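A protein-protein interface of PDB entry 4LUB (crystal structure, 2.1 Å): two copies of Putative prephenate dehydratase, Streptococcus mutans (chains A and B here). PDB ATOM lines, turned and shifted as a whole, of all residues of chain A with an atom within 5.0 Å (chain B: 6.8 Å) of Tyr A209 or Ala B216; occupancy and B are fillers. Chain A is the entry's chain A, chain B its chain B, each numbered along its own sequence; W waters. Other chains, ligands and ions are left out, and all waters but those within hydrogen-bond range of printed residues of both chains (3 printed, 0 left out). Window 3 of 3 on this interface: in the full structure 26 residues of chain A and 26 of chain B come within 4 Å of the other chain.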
ATOM      1  N   GLY A 206       1.663 -12.877  19.999  1.00  0.00           N
ATOM      2  CA  GLY A 206       2.909 -12.282  20.462  1.00  0.00           C
ATOM      3  C   GLY A 206       2.878 -10.884  21.065  1.00  0.00           C
ATOM      4  O   GLY A 206       3.758 -10.539  21.844  1.00  0.00           O
ATOM      5  N   ALA A 207       1.858 -10.091  20.757  1.00  0.00           N
ATOM      6  CA  ALA A 207       1.795  -8.713  21.259  1.00  0.00           C
ATOM      7  C   ALA A 207       0.871  -8.583  22.471  1.00  0.00           C
ATOM      8  O   ALA A 207       0.576  -7.473  22.899  1.00  0.00           O
ATOM      9  CB  ALA A 207       1.332  -7.759  20.154  1.00  0.00           C
ATOM     10  N   LEU A 208       0.399  -9.710  23.004  1.00  0.00           N
ATOM     11  CA  LEU A 208      -0.426  -9.711  24.220  1.00  0.00           C
ATOM     12  C   LEU A 208       0.199  -8.992  25.412  1.00  0.00           C
ATOM     13  O   LEU A 208      -0.491  -8.264  26.126  1.00  0.00           O
ATOM     14  CB  LEU A 208      -0.766 -11.147  24.636  1.00  0.00           C
ATOM     15  CG  LEU A 208      -1.848 -11.286  25.714  1.00  0.00           C
ATOM     16  CD1 LEU A 208      -3.121 -10.502  25.356  1.00  0.00           C
ATOM     17  CD2 LEU A 208      -2.166 -12.753  25.934  1.00  0.00           C
ATOM     18  N   TYR A 209       1.486  -9.237  25.647  1.00  0.00           N
ATOM     19  CA  TYR A 209       2.217  -8.551  26.711  1.00  0.00           C
ATOM     20  C   TYR A 209       2.034  -7.036  26.669  1.00  0.00           C
ATOM     21  O   TYR A 209       2.007  -6.398  27.713  1.00  0.00           O
ATOM     22  CB  TYR A 209       3.713  -8.910  26.676  1.00  0.00           C
ATOM     23  CG  TYR A 209       4.538  -8.144  25.664  1.00  0.00           C
ATOM     24  CD1 TYR A 209       4.515  -8.496  24.315  1.00  0.00           C
ATOM     25  CD2 TYR A 209       5.330  -7.066  26.048  1.00  0.00           C
ATOM     26  CE1 TYR A 209       5.271  -7.813  23.381  1.00  0.00           C
ATOM     27  CE2 TYR A 209       6.082  -6.363  25.112  1.00  0.00           C
ATOM     28  CZ  TYR A 209       6.047  -6.745  23.785  1.00  0.00           C
ATOM     29  OH  TYR A 209       6.784  -6.061  22.854  1.00  0.00           O
ATOM     30  N   LYS A 210       1.924  -6.465  25.472  1.00  0.00           N
ATOM     31  CA  LYS A 210       1.639  -5.030  25.310  1.00  0.00           C
ATOM     32  C   LYS A 210       0.275  -4.594  25.858  1.00  0.00           C
ATOM     33  O   LYS A 210       0.157  -3.544  26.502  1.00  0.00           O
ATOM     34  CB  LYS A 210       1.732  -4.630  23.832  1.00  0.00           C
ATOM     35  CG  LYS A 210       3.113  -4.808  23.217  1.00  0.00           C
ATOM     36  CD  LYS A 210       3.225  -4.085  21.887  1.00  0.00           C
ATOM     37  CE  LYS A 210       4.439  -4.561  21.112  1.00  0.00           C
ATOM     38  NZ  LYS A 210       4.802  -3.600  20.045  1.00  0.00           N
ATOM     39  N   ALA A 211      -0.750  -5.392  25.582  1.00  0.00           N
ATOM     40  CA  ALA A 211      -2.093  -5.116  26.076  1.00  0.00           C
ATOM     41  C   ALA A 211      -2.121  -5.200  27.598  1.00  0.00           C
ATOM     42  O   ALA A 211      -2.708  -4.349  28.272  1.00  0.00           O
ATOM     43  CB  ALA A 211      -3.099  -6.091  25.465  1.00  0.00           C
ATOM     44  N   LEU A 212      -1.504  -6.245  28.136  1.00  0.00           N
ATOM     45  CA  LEU A 212      -1.411  -6.393  29.588  1.00  0.00           C
ATOM     46  C   LEU A 212      -0.561  -5.313  30.267  1.00  0.00           C
ATOM     47  O   LEU A 212      -0.908  -4.832  31.342  1.00  0.00           O
ATOM     48  CB  LEU A 212      -0.856  -7.778  29.934  1.00  0.00           C
ATOM     49  CG  LEU A 212      -1.823  -8.977  29.936  1.00  0.00           C
ATOM     50  CD1 LEU A 212      -2.933  -8.920  28.875  1.00  0.00           C
ATOM     51  CD2 LEU A 212      -1.044 -10.263  29.850  1.00  0.00           C
ATOM     52  N   SER A 213       0.558  -4.944  29.652  1.00  0.00           N
ATOM     53  CA  SER A 213       1.398  -3.874  30.190  1.00  0.00           C
ATOM     54  C   SER A 213       0.650  -2.538  30.254  1.00  0.00           C
ATOM     55  O   SER A 213       0.879  -1.732  31.156  1.00  0.00           O
ATOM     56  CB  SER A 213       2.672  -3.702  29.364  1.00  0.00           C
ATOM     57  OG  SER A 213       3.478  -4.868  29.431  1.00  0.00           O
ATOM     58  N   THR A 214      -0.212  -2.296  29.272  1.00  0.00           N
ATOM     59  CA  THR A 214      -1.039  -1.085  29.225  1.00  0.00           C
ATOM     60  C   THR A 214      -1.868  -0.911  30.489  1.00  0.00           C
ATOM     61  O   THR A 214      -1.978   0.187  31.021  1.00  0.00           O
ATOM     62  CB  THR A 214      -1.968  -1.091  27.987  1.00  0.00           C
ATOM     63  OG1 THR A 214      -1.171  -0.999  26.797  1.00  0.00           O
ATOM     64  CG2 THR A 214      -2.936   0.082  28.021  1.00  0.00           C
ATOM     65  N   TYR B 209       1.221 -10.366  33.141  1.00  0.00           N
ATOM     66  CA  TYR B 209       2.118  -9.479  32.409  1.00  0.00           C
ATOM     67  C   TYR B 209       3.604  -9.645  32.769  1.00  0.00           C
ATOM     68  O   TYR B 209       4.457  -9.553  31.894  1.00  0.00           O
ATOM     69  CB  TYR B 209       1.678  -8.028  32.597  1.00  0.00           C
ATOM     70  CG  TYR B 209       2.156  -7.373  33.859  1.00  0.00           C
ATOM     71  CD1 TYR B 209       1.531  -7.627  35.073  1.00  0.00           C
ATOM     72  CD2 TYR B 209       3.235  -6.502  33.845  1.00  0.00           C
ATOM     73  CE1 TYR B 209       1.954  -7.017  36.236  1.00  0.00           C
ATOM     74  CE2 TYR B 209       3.674  -5.891  35.007  1.00  0.00           C
ATOM     75  CZ  TYR B 209       3.029  -6.153  36.200  1.00  0.00           C
ATOM     76  OH  TYR B 209       3.455  -5.558  37.368  1.00  0.00           O
ATOM     77  N   ALA B 211       5.001 -12.456  33.759  1.00  0.00           N
ATOM     78  CA  ALA B 211       5.393 -13.708  33.137  1.00  0.00           C
ATOM     79  C   ALA B 211       5.619 -13.544  31.640  1.00  0.00           C
ATOM     80  O   ALA B 211       6.612 -14.021  31.102  1.00  0.00           O
ATOM     81  CB  ALA B 211       4.336 -14.784  33.409  1.00  0.00           C
ATOM     82  N   LEU B 212       4.694 -12.880  30.959  1.00  0.00           N
ATOM     83  CA  LEU B 212       4.863 -12.619  29.531  1.00  0.00           C
ATOM     84  C   LEU B 212       6.009 -11.662  29.183  1.00  0.00           C
ATOM     85  O   LEU B 212       6.676 -11.851  28.170  1.00  0.00           O
ATOM     86  CB  LEU B 212       3.558 -12.100  28.923  1.00  0.00           C
ATOM     87  CG  LEU B 212       2.521 -13.160  28.496  1.00  0.00           C
ATOM     88  CD1 LEU B 212       2.513 -14.391  29.387  1.00  0.00           C
ATOM     89  CD2 LEU B 212       1.136 -12.556  28.370  1.00  0.00           C
ATOM     90  N   SER B 213       6.219 -10.629  29.994  1.00  0.00           N
ATOM     91  CA  SER B 213       7.323  -9.687  29.753  1.00  0.00           C
ATOM     92  C   SER B 213       8.681 -10.375  29.765  1.00  0.00           C
ATOM     93  O   SER B 213       9.590  -9.999  29.023  1.00  0.00           O
ATOM     94  CB  SER B 213       7.310  -8.558  30.787  1.00  0.00           C
ATOM     95  OG  SER B 213       6.136  -7.771  30.654  1.00  0.00           O
ATOM     96  N   THR B 214       8.799 -11.384  30.618  1.00  0.00           N
ATOM     97  CA  THR B 214      10.009 -12.181  30.754  1.00  0.00           C
ATOM     98  C   THR B 214      10.464 -12.747  29.405  1.00  0.00           C
ATOM     99  O   THR B 214      11.648 -12.724  29.067  1.00  0.00           O
ATOM    100  CB  THR B 214       9.786 -13.338  31.746  1.00  0.00           C
ATOM    101  OG1 THR B 214       9.540 -12.812  33.059  1.00  0.00           O
ATOM    102  CG2 THR B 214      10.989 -14.228  31.788  1.00  0.00           C
ATOM    103  N   PHE B 215       9.511 -13.276  28.650  1.00  0.00           N
ATOM    104  CA  PHE B 215       9.777 -13.785  27.313  1.00  0.00           C
ATOM    105  C   PHE B 215       9.809 -12.674  26.275  1.00  0.00           C
ATOM    106  O   PHE B 215      10.611 -12.707  25.337  1.00  0.00           O
ATOM    107  CB  PHE B 215       8.731 -14.831  26.929  1.00  0.00           C
ATOM    108  CG  PHE B 215       8.845 -16.110  27.706  1.00  0.00           C
ATOM    109  CD1 PHE B 215       8.213 -16.254  28.931  1.00  0.00           C
ATOM    110  CD2 PHE B 215       9.588 -17.170  27.211  1.00  0.00           C
ATOM    111  CE1 PHE B 215       8.323 -17.434  29.649  1.00  0.00           C
ATOM    112  CE2 PHE B 215       9.701 -18.354  27.925  1.00  0.00           C
ATOM    113  CZ  PHE B 215       9.066 -18.480  29.142  1.00  0.00           C
ATOM    114  N   ALA B 216       8.903 -11.713  26.435  1.00  0.00           N
ATOM    115  CA  ALA B 216       8.786 -10.598  25.508  1.00  0.00           C
ATOM    116  C   ALA B 216      10.062  -9.775  25.362  1.00  0.00           C
ATOM    117  O   ALA B 216      10.506  -9.525  24.240  1.00  0.00           O
ATOM    118  CB  ALA B 216       7.632  -9.688  25.929  1.00  0.00           C
ATOM    119  N   TRP B 217      10.654  -9.351  26.476  1.00  0.00           N
ATOM    120  CA  TRP B 217      11.850  -8.510  26.373  1.00  0.00           C
ATOM    121  C   TRP B 217      12.990  -9.257  25.691  1.00  0.00           C
ATOM    122  O   TRP B 217      13.812  -8.632  25.031  1.00  0.00           O
ATOM    123  CB  TRP B 217      12.269  -7.925  27.751  1.00  0.00           C
ATOM    124  CG  TRP B 217      13.051  -8.794  28.748  1.00  0.00           C
ATOM    125  CD1 TRP B 217      12.555  -9.375  29.884  1.00  0.00           C
ATOM    126  CD2 TRP B 217      14.451  -9.136  28.706  1.00  0.00           C
ATOM    127  NE1 TRP B 217      13.556 -10.067  30.545  1.00  0.00           N
ATOM    128  CE2 TRP B 217      14.721  -9.940  29.840  1.00  0.00           C
ATOM    129  CE3 TRP B 217      15.491  -8.859  27.815  1.00  0.00           C
ATOM    130  CZ2 TRP B 217      15.990 -10.451  30.107  1.00  0.00           C
ATOM    131  CZ3 TRP B 217      16.757  -9.376  28.087  1.00  0.00           C
ATOM    132  CH2 TRP B 217      16.990 -10.162  29.220  1.00  0.00           C
ATOM    133  N   ARG B 218      12.996 -10.588  25.772  1.00  0.00           N
ATOM    134  CA  ARG B 218      14.032 -11.369  25.099  1.00  0.00           C
ATOM    135  C   ARG B 218      13.672 -11.645  23.641  1.00  0.00           C
ATOM    136  O   ARG B 218      14.432 -12.291  22.924  1.00  0.00           O
ATOM    137  CB  ARG B 218      14.272 -12.711  25.814  1.00  0.00           C
ATOM    138  CG  ARG B 218      14.615 -12.613  27.295  1.00  0.00           C
ATOM    139  CD  ARG B 218      14.925 -13.991  27.878  1.00  0.00           C
ATOM    140  NE  ARG B 218      15.748 -13.901  29.083  1.00  0.00           N
ATOM    141  CZ  ARG B 218      15.286 -13.626  30.298  1.00  0.00           C
ATOM    142  NH1 ARG B 218      13.987 -13.429  30.507  1.00  0.00           N
ATOM    143  NH2 ARG B 218      16.126 -13.560  31.312  1.00  0.00           N
ATOM    144  N   GLY B 219      12.521 -11.145  23.202  1.00  0.00           N
ATOM    145  CA  GLY B 219      12.048 -11.422  21.859  1.00  0.00           C
ATOM    146  C   GLY B 219      11.624 -12.858  21.574  1.00  0.00           C
ATOM    147  O   GLY B 219      11.617 -13.283  20.419  1.00  0.00           O
ATOM    148  N   ILE B 220      11.291 -13.614  22.614  1.00  0.00           N
ATOM    149  CA  ILE B 220      10.726 -14.955  22.426  1.00  0.00           C
ATOM    150  C   ILE B 220       9.214 -14.829  22.247  1.00  0.00           C
ATOM    151  O   ILE B 220       8.507 -14.451  23.181  1.00  0.00           O
ATOM    152  CB  ILE B 220      11.054 -15.888  23.605  1.00  0.00           C
ATOM    153  CG1 ILE B 220      12.578 -16.061  23.738  1.00  0.00           C
ATOM    154  CG2 ILE B 220      10.372 -17.254  23.434  1.00  0.00           C
ATOM    155  CD1 ILE B 220      13.028 -16.487  25.132  1.00  0.00           C
ATOM    156  N   ASP B 221       8.721 -15.143  21.051  1.00  0.00           N
ATOM    157  CA  ASP B 221       7.307 -14.908  20.714  1.00  0.00           C
ATOM    158  C   ASP B 221       6.338 -15.901  21.336  1.00  0.00           C
ATOM    159  O   ASP B 221       6.502 -17.109  21.203  1.00  0.00           O
ATOM    160  CB  ASP B 221       7.091 -14.918  19.195  1.00  0.00           C
ATOM    161  CG  ASP B 221       7.768 -13.753  18.505  1.00  0.00           C
ATOM    162  OD1 ASP B 221       7.864 -12.678  19.123  1.00  0.00           O
ATOM    163  OD2 ASP B 221       8.159 -13.902  17.336  1.00  0.00           O
ATOM    164  N   LEU B 222       5.319 -15.356  21.989  1.00  0.00           N
ATOM    165  CA  LEU B 222       4.182 -16.119  22.480  1.00  0.00           C
ATOM    166  C   LEU B 222       3.297 -16.469  21.292  1.00  0.00           C
ATOM    167  O   LEU B 222       2.929 -15.594  20.506  1.00  0.00           O
ATOM    168  CB  LEU B 222       3.410 -15.293  23.519  1.00  0.00           C
ATOM    169  CG  LEU B 222       2.260 -15.793  24.418  1.00  0.00           C
ATOM    170  CD1 LEU B 222       0.980 -16.014  23.649  1.00  0.00           C
ATOM    171  CD2 LEU B 222       2.627 -17.033  25.199  1.00  0.00           C
ATOM    172  N   PHE B 243       5.564 -20.977  23.368  1.00  0.00           N
ATOM    173  CA  PHE B 243       6.551 -20.029  22.877  1.00  0.00           C
ATOM    174  C   PHE B 243       7.386 -20.713  21.822  1.00  0.00           C
ATOM    175  O   PHE B 243       7.585 -21.927  21.864  1.00  0.00           O
ATOM    176  CB  PHE B 243       7.483 -19.551  23.998  1.00  0.00           C
ATOM    177  CG  PHE B 243       6.854 -18.586  24.956  1.00  0.00           C
ATOM    178  CD1 PHE B 243       6.620 -17.277  24.583  1.00  0.00           C
ATOM    179  CD2 PHE B 243       6.523 -18.978  26.239  1.00  0.00           C
ATOM    180  CE1 PHE B 243       6.046 -16.383  25.460  1.00  0.00           C
ATOM    181  CE2 PHE B 243       5.954 -18.077  27.116  1.00  0.00           C
ATOM    182  CZ  PHE B 243       5.713 -16.781  26.728  1.00  0.00           C
HETATM  183  O   HOH W   1       2.842 -14.623  18.004  1.00  0.00           O
HETATM  184  O   HOH W   2       6.498  -5.359  29.659  1.00  0.00           O
HETATM  185  O   HOH W   3       6.880 -10.853  21.852  1.00  0.00           O
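O of Leu B222 sits at hydrogen-bond distance from N of Gly A206, 3.0 Å away.
The backbone carbonyl oxygen of Tyr A209 is in hydrogen-bond range of the side-chain hydroxyl of Ser A213 (2.7 Å). O of Tyr B209 lies within hydrogen-bond range of OG of Ser B213, at 2.7 Å.
CB of Tyr A209 touches CB of Leu B212 (3.9 Å). CG of Tyr A209 touches CB of Ala B216, 3.5 Å away. CB of Leu A212 touches CB of Tyr B209, 3.7 Å away. Leu A212 touches Leu B212 (CD2 to CD2, 3.5 Å).
Of the printed residues of chain B, Gly A206 touches Leu B222. Of chain B, only Leu B212 (3.9 Å) and Ala B216 (3.5 Å) come within 4 Å of Tyr A209. Ala A211 touches none of the printed residues of chain B. Of the printed residues of chain B, Leu A212 touches Tyr B209 (3.7 Å) and Leu B212 (3.5 Å). Of the printed residues of chain A, Tyr B209 touches Leu A212 (3.7 Å). Of the printed residues of chain A, Leu B212 touches Tyr A209 (3.9 Å) and Leu A212 (3.5 Å). Ala B216 touches just one residue of chain A: Tyr A209. Trp B217 touches none of the printed residues of chain A. Of the printed residues of chain A, Leu B222 touches Gly A206. The nearest printed residue of chain A that does not touch Ala B216 is Gly A206 (5.7 Å). The nearest printed residue of chain A that does not touch Tyr B209 is Ser A213 (4.4 Å).
Of the 9 printed residues of chain A, 3 touch a printed residue of chain B. Printed residues of chain A that touch a printed residue of chain B: Gly A206, Tyr A209 and Leu A212.
Tyr A209 touches Leu B212, and with the chains exchanged Leu A212 touches Tyr B209. Leu B212 touches its own counterpart, Leu A212. Positions printed for both chains: 209, 211, 212, 213 and 214.
Water W2 lies within hydrogen-bond range of the side-chain hydroxyl of Ser B213 (2.6 Å) and the side-chain hydroxyl of Ser A213 (3.1 Å). Water W1 lies within hydrogen-bond range of O of Leu B222 and N of Gly A206. Water W3 lies within hydrogen-bond range of O of Gly A206 and OD1 of Asp B221.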
